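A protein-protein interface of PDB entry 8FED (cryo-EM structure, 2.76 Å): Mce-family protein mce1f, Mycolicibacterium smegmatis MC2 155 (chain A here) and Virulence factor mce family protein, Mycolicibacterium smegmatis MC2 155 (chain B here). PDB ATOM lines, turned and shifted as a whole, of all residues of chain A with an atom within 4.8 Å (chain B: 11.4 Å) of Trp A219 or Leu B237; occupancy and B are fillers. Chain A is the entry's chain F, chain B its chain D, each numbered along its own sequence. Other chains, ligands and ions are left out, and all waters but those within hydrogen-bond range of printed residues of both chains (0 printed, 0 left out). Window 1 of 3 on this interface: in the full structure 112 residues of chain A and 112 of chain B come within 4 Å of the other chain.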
ATOM      1  N   ALA A 215      14.421 -16.128  -0.828  1.00  0.00           N
ATOM      2  CA  ALA A 215      15.646 -15.924  -1.593  1.00  0.00           C
ATOM      3  C   ALA A 215      16.879 -15.939  -0.698  1.00  0.00           C
ATOM      4  O   ALA A 215      17.902 -16.540  -1.053  1.00  0.00           O
ATOM      5  CB  ALA A 215      15.567 -14.614  -2.373  1.00  0.00           C
ATOM      6  N   ILE A 216      16.814 -15.277   0.461  1.00  0.00           N
ATOM      7  CA  ILE A 216      17.992 -15.236   1.324  1.00  0.00           C
ATOM      8  C   ILE A 216      18.258 -16.606   1.933  1.00  0.00           C
ATOM      9  O   ILE A 216      19.415 -17.028   2.041  1.00  0.00           O
ATOM     10  CB  ILE A 216      17.891 -14.129   2.391  1.00  0.00           C
ATOM     11  CG1 ILE A 216      16.559 -14.150   3.126  1.00  0.00           C
ATOM     12  CG2 ILE A 216      18.138 -12.767   1.765  1.00  0.00           C
ATOM     13  CD1 ILE A 216      16.353 -12.943   4.015  1.00  0.00           C
ATOM     14  N   GLN A 217      17.203 -17.334   2.314  1.00  0.00           N
ATOM     15  CA  GLN A 217      17.401 -18.703   2.785  1.00  0.00           C
ATOM     16  C   GLN A 217      18.021 -19.582   1.702  1.00  0.00           C
ATOM     17  O   GLN A 217      18.939 -20.369   1.976  1.00  0.00           O
ATOM     18  CB  GLN A 217      16.076 -19.297   3.259  1.00  0.00           C
ATOM     19  CG  GLN A 217      15.522 -18.660   4.519  1.00  0.00           C
ATOM     20  CD  GLN A 217      14.220 -19.294   4.963  1.00  0.00           C
ATOM     21  OE1 GLN A 217      13.789 -20.304   4.407  1.00  0.00           O
ATOM     22  NE2 GLN A 217      13.586 -18.703   5.967  1.00  0.00           N
ATOM     23  N   ARG A 218      17.539 -19.454   0.463  1.00  0.00           N
ATOM     24  CA  ARG A 218      18.052 -20.274  -0.631  1.00  0.00           C
ATOM     25  C   ARG A 218      19.517 -19.974  -0.926  1.00  0.00           C
ATOM     26  O   ARG A 218      20.326 -20.896  -1.085  1.00  0.00           O
ATOM     27  CB  ARG A 218      17.198 -20.063  -1.880  1.00  0.00           C
ATOM     28  CG  ARG A 218      17.669 -20.843  -3.094  1.00  0.00           C
ATOM     29  CD  ARG A 218      17.645 -22.338  -2.838  1.00  0.00           C
ATOM     30  NE  ARG A 218      18.164 -23.092  -3.972  1.00  0.00           N
ATOM     31  CZ  ARG A 218      18.284 -24.412  -4.003  1.00  0.00           C
ATOM     32  NH1 ARG A 218      17.931 -25.161  -2.972  1.00  0.00           N
ATOM     33  NH2 ARG A 218      18.772 -24.994  -5.094  1.00  0.00           N
ATOM     34  N   TRP A 219      19.892 -18.691  -0.997  1.00  0.00           N
ATOM     35  CA  TRP A 219      21.299 -18.419  -1.275  1.00  0.00           C
ATOM     36  C   TRP A 219      22.183 -18.687  -0.067  1.00  0.00           C
ATOM     37  O   TRP A 219      23.363 -18.986  -0.252  1.00  0.00           O
ATOM     38  CB  TRP A 219      21.527 -16.996  -1.816  1.00  0.00           C
ATOM     39  CG  TRP A 219      21.555 -15.852  -0.836  1.00  0.00           C
ATOM     40  CD1 TRP A 219      20.571 -14.943  -0.634  1.00  0.00           C
ATOM     41  CD2 TRP A 219      22.643 -15.459   0.021  1.00  0.00           C
ATOM     42  NE1 TRP A 219      20.947 -14.030   0.318  1.00  0.00           N
ATOM     43  CE2 TRP A 219      22.217 -14.323   0.735  1.00  0.00           C
ATOM     44  CE3 TRP A 219      23.924 -15.964   0.263  1.00  0.00           C
ATOM     45  CZ2 TRP A 219      23.024 -13.685   1.673  1.00  0.00           C
ATOM     46  CZ3 TRP A 219      24.722 -15.332   1.198  1.00  0.00           C
ATOM     47  CH2 TRP A 219      24.269 -14.204   1.890  1.00  0.00           C
ATOM     48  N   ALA A 220      21.646 -18.641   1.155  1.00  0.00           N
ATOM     49  CA  ALA A 220      22.425 -19.082   2.307  1.00  0.00           C
ATOM     50  C   ALA A 220      22.734 -20.571   2.218  1.00  0.00           C
ATOM     51  O   ALA A 220      23.876 -20.996   2.439  1.00  0.00           O
ATOM     52  CB  ALA A 220      21.675 -18.760   3.599  1.00  0.00           C
ATOM     53  N   ALA A 221      21.725 -21.381   1.885  1.00  0.00           N
ATOM     54  CA  ALA A 221      21.953 -22.816   1.730  1.00  0.00           C
ATOM     55  C   ALA A 221      22.923 -23.108   0.590  1.00  0.00           C
ATOM     56  O   ALA A 221      23.800 -23.975   0.711  1.00  0.00           O
ATOM     57  CB  ALA A 221      20.625 -23.537   1.504  1.00  0.00           C
ATOM     58  N   ASN A 222      22.779 -22.397  -0.530  1.00  0.00           N
ATOM     59  CA  ASN A 222      23.680 -22.610  -1.658  1.00  0.00           C
ATOM     60  C   ASN A 222      25.104 -22.164  -1.338  1.00  0.00           C
ATOM     61  O   ASN A 222      26.068 -22.789  -1.794  1.00  0.00           O
ATOM     62  CB  ASN A 222      23.151 -21.890  -2.892  1.00  0.00           C
ATOM     63  CG  ASN A 222      21.817 -22.431  -3.347  1.00  0.00           C
ATOM     64  OD1 ASN A 222      21.199 -23.249  -2.668  1.00  0.00           O
ATOM     65  ND2 ASN A 222      21.362 -21.977  -4.505  1.00  0.00           N
ATOM     66  N   LEU A 223      25.258 -21.075  -0.580  1.00  0.00           N
ATOM     67  CA  LEU A 223      26.582 -20.675  -0.121  1.00  0.00           C
ATOM     68  C   LEU A 223      27.186 -21.741   0.776  1.00  0.00           C
ATOM     69  O   LEU A 223      28.379 -22.042   0.674  1.00  0.00           O
ATOM     70  CB  LEU A 223      26.506 -19.337   0.615  1.00  0.00           C
ATOM     71  CG  LEU A 223      27.788 -18.902   1.330  1.00  0.00           C
ATOM     72  CD1 LEU A 223      28.900 -18.627   0.329  1.00  0.00           C
ATOM     73  CD2 LEU A 223      27.536 -17.691   2.212  1.00  0.00           C
ATOM     74  N   GLN B 228      13.360  -1.800  -3.042  1.00  0.00           N
ATOM     75  CA  GLN B 228      13.098  -2.711  -4.149  1.00  0.00           C
ATOM     76  C   GLN B 228      14.401  -3.200  -4.761  1.00  0.00           C
ATOM     77  O   GLN B 228      14.488  -4.348  -5.209  1.00  0.00           O
ATOM     78  CB  GLN B 228      12.225  -2.028  -5.201  1.00  0.00           C
ATOM     79  CG  GLN B 228      10.927  -1.438  -4.660  1.00  0.00           C
ATOM     80  CD  GLN B 228       9.950  -2.491  -4.167  1.00  0.00           C
ATOM     81  OE1 GLN B 228      10.079  -3.675  -4.477  1.00  0.00           O
ATOM     82  NE2 GLN B 228       8.960  -2.058  -3.395  1.00  0.00           N
ATOM     83  N   GLN B 229      15.420  -2.338  -4.811  1.00  0.00           N
ATOM     84  CA  GLN B 229      16.713  -2.788  -5.309  1.00  0.00           C
ATOM     85  C   GLN B 229      17.309  -3.849  -4.395  1.00  0.00           C
ATOM     86  O   GLN B 229      18.013  -4.745  -4.863  1.00  0.00           O
ATOM     87  CB  GLN B 229      17.667  -1.603  -5.445  1.00  0.00           C
ATOM     88  CG  GLN B 229      17.108  -0.450  -6.257  1.00  0.00           C
ATOM     89  CD  GLN B 229      18.058   0.010  -7.341  1.00  0.00           C
ATOM     90  OE1 GLN B 229      19.052  -0.654  -7.632  1.00  0.00           O
ATOM     91  NE2 GLN B 229      17.759   1.155  -7.942  1.00  0.00           N
ATOM     92  N   PHE B 230      17.031  -3.768  -3.089  1.00  0.00           N
ATOM     93  CA  PHE B 230      17.483  -4.797  -2.155  1.00  0.00           C
ATOM     94  C   PHE B 230      16.767  -6.118  -2.398  1.00  0.00           C
ATOM     95  O   PHE B 230      17.388  -7.189  -2.345  1.00  0.00           O
ATOM     96  CB  PHE B 230      17.272  -4.342  -0.710  1.00  0.00           C
ATOM     97  CG  PHE B 230      18.105  -3.158  -0.315  1.00  0.00           C
ATOM     98  CD1 PHE B 230      19.228  -2.804  -1.044  1.00  0.00           C
ATOM     99  CD2 PHE B 230      17.766  -2.403   0.793  1.00  0.00           C
ATOM    100  CE1 PHE B 230      19.990  -1.717  -0.679  1.00  0.00           C
ATOM    101  CE2 PHE B 230      18.527  -1.316   1.163  1.00  0.00           C
ATOM    102  CZ  PHE B 230      19.641  -0.973   0.426  1.00  0.00           C
ATOM    103  N   VAL B 231      15.457  -6.060  -2.656  1.00  0.00           N
ATOM    104  CA  VAL B 231      14.727  -7.281  -3.001  1.00  0.00           C
ATOM    105  C   VAL B 231      15.287  -7.887  -4.283  1.00  0.00           C
ATOM    106  O   VAL B 231      15.485  -9.109  -4.381  1.00  0.00           O
ATOM    107  CB  VAL B 231      13.221  -6.987  -3.131  1.00  0.00           C
ATOM    108  CG1 VAL B 231      12.476  -8.226  -3.594  1.00  0.00           C
ATOM    109  CG2 VAL B 231      12.657  -6.498  -1.813  1.00  0.00           C
ATOM    110  N   ALA B 232      15.562  -7.041  -5.277  1.00  0.00           N
ATOM    111  CA  ALA B 232      16.159  -7.509  -6.522  1.00  0.00           C
ATOM    112  C   ALA B 232      17.535  -8.115  -6.284  1.00  0.00           C
ATOM    113  O   ALA B 232      17.888  -9.124  -6.901  1.00  0.00           O
ATOM    114  CB  ALA B 232      16.244  -6.362  -7.526  1.00  0.00           C
ATOM    115  N   LEU B 233      18.328  -7.506  -5.399  1.00  0.00           N
ATOM    116  CA  LEU B 233      19.649  -8.036  -5.074  1.00  0.00           C
ATOM    117  C   LEU B 233      19.547  -9.420  -4.456  1.00  0.00           C
ATOM    118  O   LEU B 233      20.296 -10.331  -4.824  1.00  0.00           O
ATOM    119  CB  LEU B 233      20.373  -7.085  -4.121  1.00  0.00           C
ATOM    120  CG  LEU B 233      21.607  -7.643  -3.407  1.00  0.00           C
ATOM    121  CD1 LEU B 233      22.725  -7.940  -4.392  1.00  0.00           C
ATOM    122  CD2 LEU B 233      22.081  -6.690  -2.325  1.00  0.00           C
ATOM    123  N   ASN B 234      18.628  -9.593  -3.505  1.00  0.00           N
ATOM    124  CA  ASN B 234      18.476 -10.899  -2.870  1.00  0.00           C
ATOM    125  C   ASN B 234      18.023 -11.954  -3.874  1.00  0.00           C
ATOM    126  O   ASN B 234      18.549 -13.074  -3.888  1.00  0.00           O
ATOM    127  CB  ASN B 234      17.501 -10.809  -1.700  1.00  0.00           C
ATOM    128  CG  ASN B 234      18.104 -10.130  -0.491  1.00  0.00           C
ATOM    129  OD1 ASN B 234      19.321 -10.124  -0.313  1.00  0.00           O
ATOM    130  ND2 ASN B 234      17.255  -9.565   0.356  1.00  0.00           N
ATOM    131  N   ASN B 235      17.057 -11.610  -4.732  1.00  0.00           N
ATOM    132  CA  ASN B 235      16.584 -12.574  -5.725  1.00  0.00           C
ATOM    133  C   ASN B 235      17.673 -12.919  -6.735  1.00  0.00           C
ATOM    134  O   ASN B 235      17.838 -14.090  -7.102  1.00  0.00           O
ATOM    135  CB  ASN B 235      15.344 -12.031  -6.431  1.00  0.00           C
ATOM    136  CG  ASN B 235      14.135 -11.978  -5.522  1.00  0.00           C
ATOM    137  OD1 ASN B 235      13.912 -12.879  -4.715  1.00  0.00           O
ATOM    138  ND2 ASN B 235      13.348 -10.916  -5.645  1.00  0.00           N
ATOM    139  N   ASP B 236      18.429 -11.918  -7.193  1.00  0.00           N
ATOM    140  CA  ASP B 236      19.506 -12.174  -8.141  1.00  0.00           C
ATOM    141  C   ASP B 236      20.613 -13.004  -7.508  1.00  0.00           C
ATOM    142  O   ASP B 236      21.206 -13.860  -8.170  1.00  0.00           O
ATOM    143  CB  ASP B 236      20.064 -10.858  -8.681  1.00  0.00           C
ATOM    144  CG  ASP B 236      19.070 -10.115  -9.550  1.00  0.00           C
ATOM    145  OD1 ASP B 236      18.191 -10.773 -10.147  1.00  0.00           O
ATOM    146  OD2 ASP B 236      19.167  -8.873  -9.641  1.00  0.00           O
ATOM    147  N   LEU B 237      20.913 -12.761  -6.231  1.00  0.00           N
ATOM    148  CA  LEU B 237      21.914 -13.565  -5.539  1.00  0.00           C
ATOM    149  C   LEU B 237      21.452 -15.008  -5.396  1.00  0.00           C
ATOM    150  O   LEU B 237      22.245 -15.941  -5.583  1.00  0.00           O
ATOM    151  CB  LEU B 237      22.218 -12.953  -4.172  1.00  0.00           C
ATOM    152  CG  LEU B 237      23.344 -13.586  -3.361  1.00  0.00           C
ATOM    153  CD1 LEU B 237      24.611 -13.666  -4.189  1.00  0.00           C
ATOM    154  CD2 LEU B 237      23.585 -12.777  -2.102  1.00  0.00           C
ATOM    155  N   ALA B 238      20.172 -15.212  -5.068  1.00  0.00           N
ATOM    156  CA  ALA B 238      19.638 -16.568  -4.987  1.00  0.00           C
ATOM    157  C   ALA B 238      19.728 -17.276  -6.331  1.00  0.00           C
ATOM    158  O   ALA B 238      20.117 -18.448  -6.396  1.00  0.00           O
ATOM    159  CB  ALA B 238      18.194 -16.535  -4.492  1.00  0.00           C
ATOM    160  N   GLN B 239      19.385 -16.581  -7.418  1.00  0.00           N
ATOM    161  CA  GLN B 239      19.485 -17.182  -8.747  1.00  0.00           C
ATOM    162  C   GLN B 239      20.934 -17.490  -9.118  1.00  0.00           C
ATOM    163  O   GLN B 239      21.232 -18.556  -9.671  1.00  0.00           O
ATOM    164  CB  GLN B 239      18.846 -16.261  -9.784  1.00  0.00           C
ATOM    165  CG  GLN B 239      18.995 -16.738 -11.215  1.00  0.00           C
ATOM    166  CD  GLN B 239      18.519 -15.710 -12.218  1.00  0.00           C
ATOM    167  OE1 GLN B 239      17.859 -14.736 -11.858  1.00  0.00           O
ATOM    168  NE2 GLN B 239      18.859 -15.917 -13.484  1.00  0.00           N
ATOM    169  N   PHE B 240      21.848 -16.562  -8.824  1.00  0.00           N
ATOM    170  CA  PHE B 240      23.255 -16.752  -9.156  1.00  0.00           C
ATOM    171  C   PHE B 240      23.849 -17.931  -8.398  1.00  0.00           C
ATOM    172  O   PHE B 240      24.659 -18.688  -8.945  1.00  0.00           O
ATOM    173  CB  PHE B 240      24.031 -15.469  -8.857  1.00  0.00           C
ATOM    174  CG  PHE B 240      25.497 -15.558  -9.151  1.00  0.00           C
ATOM    175  CD1 PHE B 240      25.963 -15.476 -10.450  1.00  0.00           C
ATOM    176  CD2 PHE B 240      26.414 -15.704  -8.125  1.00  0.00           C
ATOM    177  CE1 PHE B 240      27.314 -15.553 -10.722  1.00  0.00           C
ATOM    178  CE2 PHE B 240      27.768 -15.780  -8.391  1.00  0.00           C
ATOM    179  CZ  PHE B 240      28.217 -15.703  -9.691  1.00  0.00           C
ATOM    180  N   THR B 241      23.465 -18.098  -7.132  1.00  0.00           N
ATOM    181  CA  THR B 241      23.932 -19.251  -6.370  1.00  0.00           C
ATOM    182  C   THR B 241      23.262 -20.541  -6.836  1.00  0.00           C
ATOM    183  O   THR B 241      23.893 -21.604  -6.836  1.00  0.00           O
ATOM    184  CB  THR B 241      23.696 -19.022  -4.879  1.00  0.00           C
ATOM    185  OG1 THR B 241      22.324 -18.676  -4.657  1.00  0.00           O
ATOM    186  CG2 THR B 241      24.591 -17.908  -4.363  1.00  0.00           C
ATOM    187  N   ASN B 242      21.984 -20.472  -7.232  1.00  0.00           N
ATOM    188  CA  ASN B 242      21.324 -21.632  -7.826  1.00  0.00           C
ATOM    189  C   ASN B 242      21.997 -22.061  -9.120  1.00  0.00           C
ATOM    190  O   ASN B 242      21.931 -23.237  -9.494  1.00  0.00           O
ATOM    191  CB  ASN B 242      19.850 -21.322  -8.092  1.00  0.00           C
ATOM    192  CG  ASN B 242      18.993 -21.435  -6.851  1.00  0.00           C
ATOM    193  OD1 ASN B 242      19.503 -21.560  -5.740  1.00  0.00           O
ATOM    194  ND2 ASN B 242      17.679 -21.391  -7.034  1.00  0.00           N
ATOM    195  N   SER B 243      22.637 -21.124  -9.820  1.00  0.00           N
ATOM    196  CA  SER B 243      23.328 -21.457 -11.060  1.00  0.00           C
ATOM    197  C   SER B 243      24.518 -22.388 -10.850  1.00  0.00           C
ATOM    198  O   SER B 243      25.025 -22.941 -11.831  1.00  0.00           O
ATOM    199  CB  SER B 243      23.797 -20.182 -11.762  1.00  0.00           C
ATOM    200  OG  SER B 243      22.698 -19.373 -12.138  1.00  0.00           O
ATOM    201  N   PHE B 244      24.980 -22.573  -9.612  1.00  0.00           N
ATOM    202  CA  PHE B 244      26.127 -23.425  -9.336  1.00  0.00           C
ATOM    203  C   PHE B 244      25.821 -24.583  -8.395  1.00  0.00           C
ATOM    204  O   PHE B 244      26.734 -25.353  -8.076  1.00  0.00           O
ATOM    205  CB  PHE B 244      27.278 -22.594  -8.755  1.00  0.00           C
ATOM    206  CG  PHE B 244      27.799 -21.542  -9.689  1.00  0.00           C
ATOM    207  CD1 PHE B 244      28.497 -21.895 -10.830  1.00  0.00           C
ATOM    208  CD2 PHE B 244      27.599 -20.200  -9.423  1.00  0.00           C
ATOM    209  CE1 PHE B 244      28.980 -20.931 -11.691  1.00  0.00           C
ATOM    210  CE2 PHE B 244      28.079 -19.231 -10.279  1.00  0.00           C
ATOM    211  CZ  PHE B 244      28.771 -19.597 -11.415  1.00  0.00           C
ATOM    212  N   THR B 245      24.580 -24.731  -7.938  1.00  0.00           N
ATOM    213  CA  THR B 245      24.198 -25.801  -7.022  1.00  0.00           C
ATOM    214  C   THR B 245      23.027 -26.597  -7.574  1.00  0.00           C
ATOM    215  O   THR B 245      22.105 -26.969  -6.842  1.00  0.00           O
ATOM    216  CB  THR B 245      23.851 -25.256  -5.637  1.00  0.00           C
ATOM    217  OG1 THR B 245      22.721 -24.380  -5.735  1.00  0.00           O
ATOM    218  CG2 THR B 245      25.025 -24.501  -5.044  1.00  0.00           C
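The side-chain hydroxyl (OG1) of Thr B241 is in hydrogen-bond range of the backbone carbonyl oxygen (O) of Ala B238. The backbone carbonyl oxygen (O) of Leu B237 is in hydrogen-bond range of the side-chain hydroxyl (OG1) of Thr B241 (2.9 Å). The side-chain amide oxygen (OD1) of Asn A222 sits close to the backbone carbonyl oxygen (O) of Arg A218, 3.0 Å away. O of Thr B241 is in hydrogen-bond range of OG1 of Thr B245 (3.2 Å). ND2 of Asn B235 lies within hydrogen-bond range of O of Val B231. O of Ala B238 sits close to OD1 of Asn B242, at 3.2 Å.
Of the 18 printed residues of chain B, 7 touch a printed residue of chain A. Of the 9 printed residues of chain A, 5 touch a printed residue of chain B. Printed residues of chain A that touch a printed residue of chain B: Ala A215, Ile A216, Arg A218, Trp A219 and Asn A222.
Among the printed residues, merely in contact across the chains: Ala A215 with Asn B234, Ala A215 with Asn B235, Ala A215 with Ala B238, Ile A216 with Asn B234, Trp A219 with Leu B237, Trp A219 with Ala B238 and Trp A219 with Thr B241.
OD1 of Asn B242 is in hydrogen-bond range of NE of Arg A218 (2.7 Å). OG1 of Thr B245 is in hydrogen-bond range of ND2 of Asn A222, 3.0 Å away. The side-chain hydroxyl of Thr B241 lies close to the side-chain amide nitrogen of Asn A222, 3.4 Å away. ND2 of Asn A222 lies close to N of Asn B242.
Of chain B, only Asn B234 (3.5 Å) comes within 4 Å of Ile A216. Gln A217 touches none of the printed residues of chain B. Printed residues of chain B within 4 Å of Arg A218: Asn B242 (2.7 Å). Of chain B, only Leu B237, Ala B238 and Thr B241 come within 4 Å of Trp A219. No residue of chain B comes within 4 Å of Ala A221. Of chain B, only Thr B241 (3.3 Å), Asn B242 (2.3 Å) and Thr B245 (3.0 Å) come within 4 Å of Asn A222. Printed residues of chain A within 4 Å of Asn B234: Ala A215 (3.7 Å) and Ile A216 (3.5 Å). Of the printed residues of chain A, Asn B235 touches Ala A215. Leu B237 touches just one residue of chain A: Trp A219. Of the printed residues of chain A, Thr B241 touches Trp A219 and Asn A222. Phe B244 touches none of the printed residues of chain A. The nearest residue of chain B that does not touch Trp A219 is Asn B234 (4.3 Å). The nearest printed residue of chain A that does not touch Leu B237 is Ala A215 (5.8 Å). The nearest printed residue of chain A that does not touch Thr B241 is Arg A218 (4.7 Å).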
